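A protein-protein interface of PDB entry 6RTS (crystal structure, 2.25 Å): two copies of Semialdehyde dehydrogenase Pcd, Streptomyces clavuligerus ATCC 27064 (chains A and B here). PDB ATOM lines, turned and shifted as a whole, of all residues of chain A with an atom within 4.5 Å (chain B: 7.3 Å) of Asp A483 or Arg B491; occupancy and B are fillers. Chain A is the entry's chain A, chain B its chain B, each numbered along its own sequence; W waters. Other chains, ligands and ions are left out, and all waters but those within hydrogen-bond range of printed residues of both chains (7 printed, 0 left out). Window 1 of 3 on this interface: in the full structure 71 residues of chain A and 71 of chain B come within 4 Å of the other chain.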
ATOM      1  N   GLY A 451      15.690   9.973  -3.828  1.00  0.00           N
ATOM      2  CA  GLY A 451      14.244  10.190  -3.992  1.00  0.00           C
ATOM      3  C   GLY A 451      13.832  11.666  -3.968  1.00  0.00           C
ATOM      4  O   GLY A 451      12.811  12.023  -4.512  1.00  0.00           O
ATOM      5  N   ALA A 467       5.524  13.434  -3.277  1.00  0.00           N
ATOM      6  CA  ALA A 467       5.755  12.070  -2.807  1.00  0.00           C
ATOM      7  C   ALA A 467       7.006  12.105  -1.968  1.00  0.00           C
ATOM      8  O   ALA A 467       8.051  12.569  -2.433  1.00  0.00           O
ATOM      9  CB  ALA A 467       5.945  11.113  -3.967  1.00  0.00           C
ATOM     10  N   GLU A 471      15.307   6.003  -2.197  1.00  0.00           N
ATOM     11  CA  GLU A 471      15.761   4.862  -2.956  1.00  0.00           C
ATOM     12  C   GLU A 471      16.857   4.106  -2.193  1.00  0.00           C
ATOM     13  O   GLU A 471      17.287   4.519  -1.104  1.00  0.00           O
ATOM     14  CB  GLU A 471      16.320   5.374  -4.299  1.00  0.00           C
ATOM     15  CG  GLU A 471      15.287   6.054  -5.180  1.00  0.00           C
ATOM     16  CD  GLU A 471      14.113   5.136  -5.446  1.00  0.00           C
ATOM     17  OE1 GLU A 471      14.351   4.029  -6.002  1.00  0.00           O
ATOM     18  OE2 GLU A 471      12.975   5.495  -5.039  1.00  0.00           O
ATOM     19  N   ARG A 478       6.971   5.462  -0.936  1.00  0.00           N
ATOM     20  CA  ARG A 478       6.544   6.868  -1.021  1.00  0.00           C
ATOM     21  C   ARG A 478       5.281   7.135  -0.167  1.00  0.00           C
ATOM     22  O   ARG A 478       4.345   6.328  -0.151  1.00  0.00           O
ATOM     23  CB  ARG A 478       6.283   7.302  -2.470  1.00  0.00           C
ATOM     24  CG  ARG A 478       7.507   7.342  -3.375  1.00  0.00           C
ATOM     25  CD  ARG A 478       8.554   8.373  -2.915  1.00  0.00           C
ATOM     26  NE  ARG A 478       9.688   8.462  -3.837  1.00  0.00           N
ATOM     27  CZ  ARG A 478      10.735   7.622  -3.886  1.00  0.00           C
ATOM     28  NH1 ARG A 478      10.856   6.571  -3.059  1.00  0.00           N
ATOM     29  NH2 ARG A 478      11.676   7.834  -4.796  1.00  0.00           N
ATOM     30  N   GLY A 481       2.175  12.936  -0.864  1.00  0.00           N
ATOM     31  CA  GLY A 481       1.683  13.581  -2.085  1.00  0.00           C
ATOM     32  C   GLY A 481       1.696  12.811  -3.404  1.00  0.00           C
ATOM     33  O   GLY A 481       1.808  11.574  -3.437  1.00  0.00           O
ATOM     34  N   SER A 482       1.571  13.568  -4.501  1.00  0.00           N
ATOM     35  CA  SER A 482       1.379  13.021  -5.852  1.00  0.00           C
ATOM     36  C   SER A 482       0.367  11.860  -5.772  1.00  0.00           C
ATOM     37  O   SER A 482      -0.622  11.986  -5.043  1.00  0.00           O
ATOM     38  CB  SER A 482       2.716  12.616  -6.449  1.00  0.00           C
ATOM     39  OG  SER A 482       2.594  12.318  -7.824  1.00  0.00           O
ATOM     40  N   ASP A 483       0.625  10.740  -6.443  1.00  0.00           N
ATOM     41  CA  ASP A 483      -0.267   9.584  -6.394  1.00  0.00           C
ATOM     42  C   ASP A 483       0.269   8.477  -5.483  1.00  0.00           C
ATOM     43  O   ASP A 483       0.057   7.295  -5.718  1.00  0.00           O
ATOM     44  CB  ASP A 483      -0.584   9.074  -7.807  1.00  0.00           C
ATOM     45  CG  ASP A 483       0.657   8.650  -8.577  1.00  0.00           C
ATOM     46  OD1 ASP A 483       1.784   8.874  -8.056  1.00  0.00           O
ATOM     47  OD2 ASP A 483       0.506   8.113  -9.708  1.00  0.00           O
ATOM     48  N   ALA A 484       0.918   8.879  -4.399  1.00  0.00           N
ATOM     49  CA  ALA A 484       1.357   7.954  -3.376  1.00  0.00           C
ATOM     50  C   ALA A 484       0.183   7.142  -2.833  1.00  0.00           C
ATOM     51  O   ALA A 484       0.396   6.024  -2.384  1.00  0.00           O
ATOM     52  CB  ALA A 484       2.066   8.703  -2.241  1.00  0.00           C
ATOM     53  N   TRP A 485      -1.032   7.706  -2.879  1.00  0.00           N
ATOM     54  CA  TRP A 485      -2.271   6.997  -2.501  1.00  0.00           C
ATOM     55  C   TRP A 485      -2.460   5.630  -3.151  1.00  0.00           C
ATOM     56  O   TRP A 485      -3.071   4.764  -2.556  1.00  0.00           O
ATOM     57  CB  TRP A 485      -3.538   7.849  -2.760  1.00  0.00           C
ATOM     58  CG  TRP A 485      -3.825   8.175  -4.209  1.00  0.00           C
ATOM     59  CD1 TRP A 485      -3.465   9.312  -4.880  1.00  0.00           C
ATOM     60  CD2 TRP A 485      -4.527   7.359  -5.156  1.00  0.00           C
ATOM     61  NE1 TRP A 485      -3.890   9.254  -6.177  1.00  0.00           N
ATOM     62  CE2 TRP A 485      -4.550   8.070  -6.380  1.00  0.00           C
ATOM     63  CE3 TRP A 485      -5.138   6.095  -5.093  1.00  0.00           C
ATOM     64  CZ2 TRP A 485      -5.163   7.560  -7.544  1.00  0.00           C
ATOM     65  CZ3 TRP A 485      -5.756   5.584  -6.254  1.00  0.00           C
ATOM     66  CH2 TRP A 485      -5.759   6.325  -7.458  1.00  0.00           C
ATOM     67  N   ARG A 486      -1.943   5.445  -4.359  1.00  0.00           N
ATOM     68  CA  ARG A 486      -2.085   4.164  -5.073  1.00  0.00           C
ATOM     69  C   ARG A 486      -1.584   2.932  -4.342  1.00  0.00           C
ATOM     70  O   ARG A 486      -2.126   1.846  -4.524  1.00  0.00           O
ATOM     71  CB  ARG A 486      -1.448   4.235  -6.458  1.00  0.00           C
ATOM     72  CG  ARG A 486      -2.250   5.124  -7.399  1.00  0.00           C
ATOM     73  CD  ARG A 486      -1.669   5.270  -8.809  1.00  0.00           C
ATOM     74  NE  ARG A 486      -2.654   5.924  -9.696  1.00  0.00           N
ATOM     75  CZ  ARG A 486      -2.754   5.755 -11.018  1.00  0.00           C
ATOM     76  NH1 ARG A 486      -1.926   4.945 -11.701  1.00  0.00           N
ATOM     77  NH2 ARG A 486      -3.709   6.407 -11.682  1.00  0.00           N
ATOM     78  N   ARG B 136       5.100  14.932 -13.087  1.00  0.00           N
ATOM     79  CA  ARG B 136       4.213  16.060 -12.792  1.00  0.00           C
ATOM     80  C   ARG B 136       4.984  17.356 -12.500  1.00  0.00           C
ATOM     81  O   ARG B 136       6.139  17.339 -12.064  1.00  0.00           O
ATOM     82  CB  ARG B 136       3.312  15.712 -11.594  1.00  0.00           C
ATOM     83  CG  ARG B 136       2.512  14.455 -11.863  1.00  0.00           C
ATOM     84  CD  ARG B 136       1.489  14.153 -10.800  1.00  0.00           C
ATOM     85  NE  ARG B 136       0.425  13.284 -11.321  1.00  0.00           N
ATOM     86  CZ  ARG B 136      -0.430  12.578 -10.568  1.00  0.00           C
ATOM     87  NH1 ARG B 136      -0.369  12.594  -9.228  1.00  0.00           N
ATOM     88  NH2 ARG B 136      -1.362  11.837 -11.159  1.00  0.00           N
ATOM     89  N   GLU B 149       7.974  16.532 -10.148  1.00  0.00           N
ATOM     90  CA  GLU B 149       8.267  15.112  -9.957  1.00  0.00           C
ATOM     91  C   GLU B 149       8.764  14.574 -11.306  1.00  0.00           C
ATOM     92  O   GLU B 149       8.092  14.745 -12.328  1.00  0.00           O
ATOM     93  CB  GLU B 149       7.014  14.387  -9.501  1.00  0.00           C
ATOM     94  CG  GLU B 149       7.136  12.879  -9.350  1.00  0.00           C
ATOM     95  CD  GLU B 149       5.769  12.230  -9.257  1.00  0.00           C
ATOM     96  OE1 GLU B 149       5.266  11.735 -10.306  1.00  0.00           O
ATOM     97  OE2 GLU B 149       5.193  12.258  -8.148  1.00  0.00           O
ATOM     98  N   THR B 150       9.943  13.944 -11.292  1.00  0.00           N
ATOM     99  CA  THR B 150      10.571  13.396 -12.494  1.00  0.00           C
ATOM    100  C   THR B 150      10.795  11.898 -12.369  1.00  0.00           C
ATOM    101  O   THR B 150      10.788  11.355 -11.259  1.00  0.00           O
ATOM    102  CB  THR B 150      11.902  14.100 -12.800  1.00  0.00           C
ATOM    103  OG1 THR B 150      12.782  13.971 -11.689  1.00  0.00           O
ATOM    104  CG2 THR B 150      11.637  15.581 -13.044  1.00  0.00           C
ATOM    105  N   TRP B 151      10.982  11.245 -13.512  1.00  0.00           N
ATOM    106  CA  TRP B 151      11.232   9.805 -13.570  1.00  0.00           C
ATOM    107  C   TRP B 151      12.537   9.504 -14.289  1.00  0.00           C
ATOM    108  O   TRP B 151      12.811  10.057 -15.355  1.00  0.00           O
ATOM    109  CB  TRP B 151      10.052   9.072 -14.238  1.00  0.00           C
ATOM    110  CG  TRP B 151       8.828   9.134 -13.384  1.00  0.00           C
ATOM    111  CD1 TRP B 151       7.924  10.126 -13.348  1.00  0.00           C
ATOM    112  CD2 TRP B 151       8.418   8.179 -12.399  1.00  0.00           C
ATOM    113  NE1 TRP B 151       6.956   9.858 -12.414  1.00  0.00           N
ATOM    114  CE2 TRP B 151       7.235   8.664 -11.815  1.00  0.00           C
ATOM    115  CE3 TRP B 151       8.943   6.969 -11.948  1.00  0.00           C
ATOM    116  CZ2 TRP B 151       6.561   7.983 -10.806  1.00  0.00           C
ATOM    117  CZ3 TRP B 151       8.258   6.279 -10.953  1.00  0.00           C
ATOM    118  CH2 TRP B 151       7.082   6.797 -10.389  1.00  0.00           C
ATOM    119  N   HIS B 152      13.345   8.638 -13.684  1.00  0.00           N
ATOM    120  CA  HIS B 152      14.663   8.294 -14.200  1.00  0.00           C
ATOM    121  C   HIS B 152      14.858   6.767 -14.375  1.00  0.00           C
ATOM    122  O   HIS B 152      14.257   5.959 -13.637  1.00  0.00           O
ATOM    123  CB  HIS B 152      15.726   8.827 -13.259  1.00  0.00           C
ATOM    124  CG  HIS B 152      15.559  10.275 -12.937  1.00  0.00           C
ATOM    125  ND1 HIS B 152      15.881  11.273 -13.828  1.00  0.00           N
ATOM    126  CD2 HIS B 152      15.084  10.894 -11.833  1.00  0.00           C
ATOM    127  CE1 HIS B 152      15.630  12.446 -13.276  1.00  0.00           C
ATOM    128  NE2 HIS B 152      15.150  12.244 -12.066  1.00  0.00           N
ATOM    129  N   LEU B 154      16.149   3.106 -13.971  1.00  0.00           N
ATOM    130  CA  LEU B 154      16.476   2.392 -12.735  1.00  0.00           C
ATOM    131  C   LEU B 154      17.820   1.650 -12.816  1.00  0.00           C
ATOM    132  O   LEU B 154      18.708   1.852 -11.994  1.00  0.00           O
ATOM    133  CB  LEU B 154      15.355   1.420 -12.450  1.00  0.00           C
ATOM    134  CG  LEU B 154      15.257   0.918 -11.033  1.00  0.00           C
ATOM    135  CD1 LEU B 154      14.879   2.048 -10.091  1.00  0.00           C
ATOM    136  CD2 LEU B 154      14.202  -0.171 -11.040  1.00  0.00           C
ATOM    137  N   ARG B 261      13.514  -4.321  -6.043  1.00  0.00           N
ATOM    138  CA  ARG B 261      12.111  -4.239  -6.417  1.00  0.00           C
ATOM    139  C   ARG B 261      11.751  -5.502  -7.201  1.00  0.00           C
ATOM    140  O   ARG B 261      12.590  -6.034  -7.934  1.00  0.00           O
ATOM    141  CB  ARG B 261      11.920  -2.987  -7.289  1.00  0.00           C
ATOM    142  CG  ARG B 261      10.476  -2.557  -7.541  1.00  0.00           C
ATOM    143  CD  ARG B 261      10.392  -1.351  -8.488  1.00  0.00           C
ATOM    144  NE  ARG B 261      11.010  -0.129  -7.932  1.00  0.00           N
ATOM    145  CZ  ARG B 261      11.079   1.053  -8.555  1.00  0.00           C
ATOM    146  NH1 ARG B 261      10.592   1.202  -9.780  1.00  0.00           N
ATOM    147  NH2 ARG B 261      11.659   2.096  -7.958  1.00  0.00           N
ATOM    148  N   ASP B 483      -0.097   2.756 -16.726  1.00  0.00           N
ATOM    149  CA  ASP B 483       1.182   3.261 -16.256  1.00  0.00           C
ATOM    150  C   ASP B 483       2.070   2.201 -15.567  1.00  0.00           C
ATOM    151  O   ASP B 483       2.813   2.511 -14.624  1.00  0.00           O
ATOM    152  CB  ASP B 483       0.924   4.467 -15.359  1.00  0.00           C
ATOM    153  CG  ASP B 483       0.221   4.111 -14.059  1.00  0.00           C
ATOM    154  OD1 ASP B 483      -0.271   2.970 -13.867  1.00  0.00           O
ATOM    155  OD2 ASP B 483       0.187   5.004 -13.203  1.00  0.00           O
ATOM    156  N   ARG B 486       5.945   2.631 -14.727  1.00  0.00           N
ATOM    157  CA  ARG B 486       6.522   3.238 -13.528  1.00  0.00           C
ATOM    158  C   ARG B 486       7.363   2.299 -12.669  1.00  0.00           C
ATOM    159  O   ARG B 486       8.254   2.769 -11.953  1.00  0.00           O
ATOM    160  CB  ARG B 486       5.444   3.882 -12.669  1.00  0.00           C
ATOM    161  CG  ARG B 486       4.843   5.065 -13.372  1.00  0.00           C
ATOM    162  CD  ARG B 486       3.898   5.861 -12.508  1.00  0.00           C
ATOM    163  NE  ARG B 486       3.782   7.156 -13.143  1.00  0.00           N
ATOM    164  CZ  ARG B 486       3.318   8.253 -12.572  1.00  0.00           C
ATOM    165  NH1 ARG B 486       2.852   8.252 -11.312  1.00  0.00           N
ATOM    166  NH2 ARG B 486       3.306   9.368 -13.291  1.00  0.00           N
ATOM    167  N   MET B 489      11.267   2.494 -13.439  1.00  0.00           N
ATOM    168  CA  MET B 489      11.955   3.777 -13.317  1.00  0.00           C
ATOM    169  C   MET B 489      11.890   4.200 -11.864  1.00  0.00           C
ATOM    170  O   MET B 489      11.138   3.618 -11.107  1.00  0.00           O
ATOM    171  CB  MET B 489      11.286   4.822 -14.212  1.00  0.00           C
ATOM    172  CG  MET B 489      11.397   4.516 -15.706  1.00  0.00           C
ATOM    173  SD  MET B 489      10.908   5.854 -16.834  1.00  0.00           S
ATOM    174  CE  MET B 489      12.362   6.881 -16.896  1.00  0.00           C
ATOM    175  N   ARG B 490      12.686   5.190 -11.473  1.00  0.00           N
ATOM    176  CA  ARG B 490      12.655   5.690 -10.086  1.00  0.00           C
ATOM    177  C   ARG B 490      12.152   7.121 -10.096  1.00  0.00           C
ATOM    178  O   ARG B 490      12.482   7.883 -10.991  1.00  0.00           O
ATOM    179  CB  ARG B 490      14.013   5.594  -9.386  1.00  0.00           C
ATOM    180  CG  ARG B 490      15.125   6.403 -10.037  1.00  0.00           C
ATOM    181  CD  ARG B 490      16.456   6.284  -9.300  1.00  0.00           C
ATOM    182  NE  ARG B 490      17.485   6.892 -10.126  1.00  0.00           N
ATOM    183  CZ  ARG B 490      17.711   8.200 -10.220  1.00  0.00           C
ATOM    184  NH1 ARG B 490      17.023   9.090  -9.485  1.00  0.00           N
ATOM    185  NH2 ARG B 490      18.656   8.636 -11.050  1.00  0.00           N
ATOM    186  N   ARG B 491      11.324   7.445  -9.106  1.00  0.00           N
ATOM    187  CA  ARG B 491      10.723   8.754  -8.945  1.00  0.00           C
ATOM    188  C   ARG B 491      11.658   9.645  -8.172  1.00  0.00           C
ATOM    189  O   ARG B 491      12.242   9.198  -7.178  1.00  0.00           O
ATOM    190  CB  ARG B 491       9.461   8.592  -8.115  1.00  0.00           C
ATOM    191  CG  ARG B 491       8.558   9.793  -8.066  1.00  0.00           C
ATOM    192  CD  ARG B 491       7.576   9.667  -6.922  1.00  0.00           C
ATOM    193  NE  ARG B 491       6.685   8.506  -7.067  1.00  0.00           N
ATOM    194  CZ  ARG B 491       5.358   8.554  -7.263  1.00  0.00           C
ATOM    195  NH1 ARG B 491       4.691   9.703  -7.364  1.00  0.00           N
ATOM    196  NH2 ARG B 491       4.670   7.421  -7.364  1.00  0.00           N
ATOM    197  N   ALA B 492      11.787  10.893  -8.619  1.00  0.00           N
ATOM    198  CA  ALA B 492      12.447  11.958  -7.846  1.00  0.00           C
ATOM    199  C   ALA B 492      11.470  13.114  -7.646  1.00  0.00           C
ATOM    200  O   ALA B 492      10.756  13.484  -8.560  1.00  0.00           O
ATOM    201  CB  ALA B 492      13.704  12.449  -8.550  1.00  0.00           C
ATOM    202  N   THR B 493      11.449  13.673  -6.449  1.00  0.00           N
ATOM    203  CA  THR B 493      10.701  14.895  -6.138  1.00  0.00           C
ATOM    204  C   THR B 493      11.729  16.044  -6.042  1.00  0.00           C
ATOM    205  O   THR B 493      12.694  15.967  -5.278  1.00  0.00           O
ATOM    206  CB  THR B 493       9.900  14.707  -4.816  1.00  0.00           C
ATOM    207  OG1 THR B 493       9.005  13.568  -4.929  1.00  0.00           O
ATOM    208  CG2 THR B 493       9.120  15.967  -4.438  1.00  0.00           C
ATOM    209  N   ASN B 494      11.564  17.083  -6.859  1.00  0.00           N
ATOM    210  CA  ASN B 494      12.557  18.142  -6.968  1.00  0.00           C
ATOM    211  C   ASN B 494      12.005  19.484  -6.586  1.00  0.00           C
ATOM    212  O   ASN B 494      11.126  19.996  -7.271  1.00  0.00           O
ATOM    213  CB  ASN B 494      13.087  18.256  -8.392  1.00  0.00           C
ATOM    214  CG  ASN B 494      13.520  16.949  -8.943  1.00  0.00           C
ATOM    215  OD1 ASN B 494      14.419  16.309  -8.404  1.00  0.00           O
ATOM    216  ND2 ASN B 494      12.878  16.527 -10.016  1.00  0.00           N
HETATM  217  O   HOH W   1       0.749   3.728 -10.482  1.00  0.00           O
HETATM  218  O   HOH W   2       6.602  13.968  -6.016  1.00  0.00           O
HETATM  219  O   HOH W   3      11.194   3.457  -5.313  1.00  0.00           O
HETATM  220  O   HOH W   4      -2.876  11.649  -7.710  1.00  0.00           O
HETATM  221  O   HOH W   5       2.554   5.537  -9.241  1.00  0.00           O
HETATM  222  O   HOH W   6      10.249  10.895  -5.255  1.00  0.00           O
HETATM  223  O   HOH W   7       2.149   5.783  -6.455  1.00  0.00           O
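Among the printed residues, merely in contact across the chains: Gly A451 with Ala B492, Ala A467 with Arg B491, Glu A471 with Arg B490 and Gly A451 with Arg B491.
Of the 10 printed residues of chain A, 7 touch a printed residue of chain B.
Hydrophobic or aromatic side chains of chain A within 4 Å of the printed part of chain B: Ala A467.
Among the printed residues, 15 pairs touch across the chains.
O of Arg B136 is in hydrogen-bond range of N of Glu B149, 2.8 Å away.
OE2 of Glu A471 is in salt-bridge range of NH2 of Arg A478, 2.7 Å away.
The backbone NH (N) of Ala B492 is in hydrogen-bond range of the backbone carbonyl oxygen (O) of Thr B150.
The guanidinium group (NE) of Arg A486 is in salt-bridge range of the side-chain carboxylate (OD2) of Asp A483 (3.8 Å).
NH1 of Arg B261 lies within hydrogen-bond range of O of Met B489, 2.8 Å away.
NE1 of Trp B151 is in hydrogen-bond range of OE1 of Glu B149.
Asp A483 touches Arg B486, and with the chains exchanged Arg A486 touches Asp B483.
Of the 15 pairs that touch across the chains among the printed residues, 2 have their exchanged pair printed and touching as well.
Printed residues of chain B within 4 Å of Ala A467: Arg B491 and Thr B493.
Printed residues of chain B within 4 Å of Ser A482: Arg B136, Glu B149 and Arg B491.
Of chain B, only Arg B136, Arg B486 and Arg B491 come within 4 Å of Asp A483.
His B152 touches none of the printed residues of chain A.
Of the printed residues of chain A, Asp B483 touches Arg A486 (2.6 Å).
Of chain A, only Gly A451 (3.9 Å), Ala A467 (3.7 Å), Arg A478 (2.8 Å), Ser A482 (3.4 Å) and Asp A483 (3.1 Å) come within 4 Å of Arg B491.
Printed residues of chain A within 4 Å of Ala B492: Gly A451 (3.4 Å).
The nearest residue of chain B that does not touch Asp A483 is Asp B483 (4.7 Å).
The nearest residue of chain A that does not touch Arg B491 is Glu A471 (4.3 Å).
The guanidinium group (NH2) of Arg A478 sits at hydrogen-bond distance from the backbone carbonyl oxygen (O) of Arg B491.
NH2 of Arg B261 lies within salt-bridge range of OE1 of Glu A471, at 3.8 Å.
The backbone carbonyl oxygen of Gly A451 is in hydrogen-bond range of the backbone NH of Thr B493 (2.9 Å).
The side-chain carboxylate (OE2) of Glu B149 sits at hydrogen-bond distance from the side-chain hydroxyl (OG) of Ser A482 (2.6 Å).
The guanidinium group (NH1) of Arg B491 is in hydrogen-bond range of the side-chain hydroxyl (OG) of Ser A482.
The guanidinium group (NH1) of Arg B491 is in salt-bridge range of the side-chain carboxylate (OD1) of Asp A483, 3.1 Å away.
The guanidinium group (NH1) of Arg A486 lies within salt-bridge range of the side-chain carboxylate (OD2) of Asp B483 (2.6 Å).
The side-chain hydroxyl (OG1) of Thr B493 is in hydrogen-bond range of the backbone carbonyl oxygen (O) of Ala A467 (2.9 Å).
NH1 of Arg B136 sits at hydrogen-bond distance from OG of Ser A482 (3.3 Å).
NH1 of Arg B136 sits close to N of Asp A483 (3.5 Å).
NH1 of Arg B486 is in salt-bridge range of OD2 of Asp A483 (2.8 Å).
Water W2 lies within hydrogen-bond range of OG1 of Thr B493, N of Ala A467 and OE2 of Glu B149.
Water W7 lies within hydrogen-bond range of the backbone carbonyl oxygen (O) of Asp A483 (2.7 Å) and the guanidinium group (NH2) of Arg B491 (3.1 Å).
Water W3 lies within hydrogen-bond range of OE2 of Glu A471 and NH2 of Arg B261.
Water W6 lies within hydrogen-bond range of the guanidinium group (NE) of Arg A478 (2.9 Å), the backbone carbonyl oxygen (O) of Gly A451 (2.9 Å), the side-chain hydroxyl (OG1) of Thr B493 (3.0 Å) and the backbone carbonyl oxygen (O) of Arg B491 (3.2 Å).
Water W1 lies within hydrogen-bond range of OD2 of Asp B483 and NH1 of Arg A486.
Water W5 lies within hydrogen-bond range of OD2 of Asp A483 (3.3 Å), NH2 of Arg B491 (3.4 Å) and NH1 of Arg B486 (3.4 Å).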
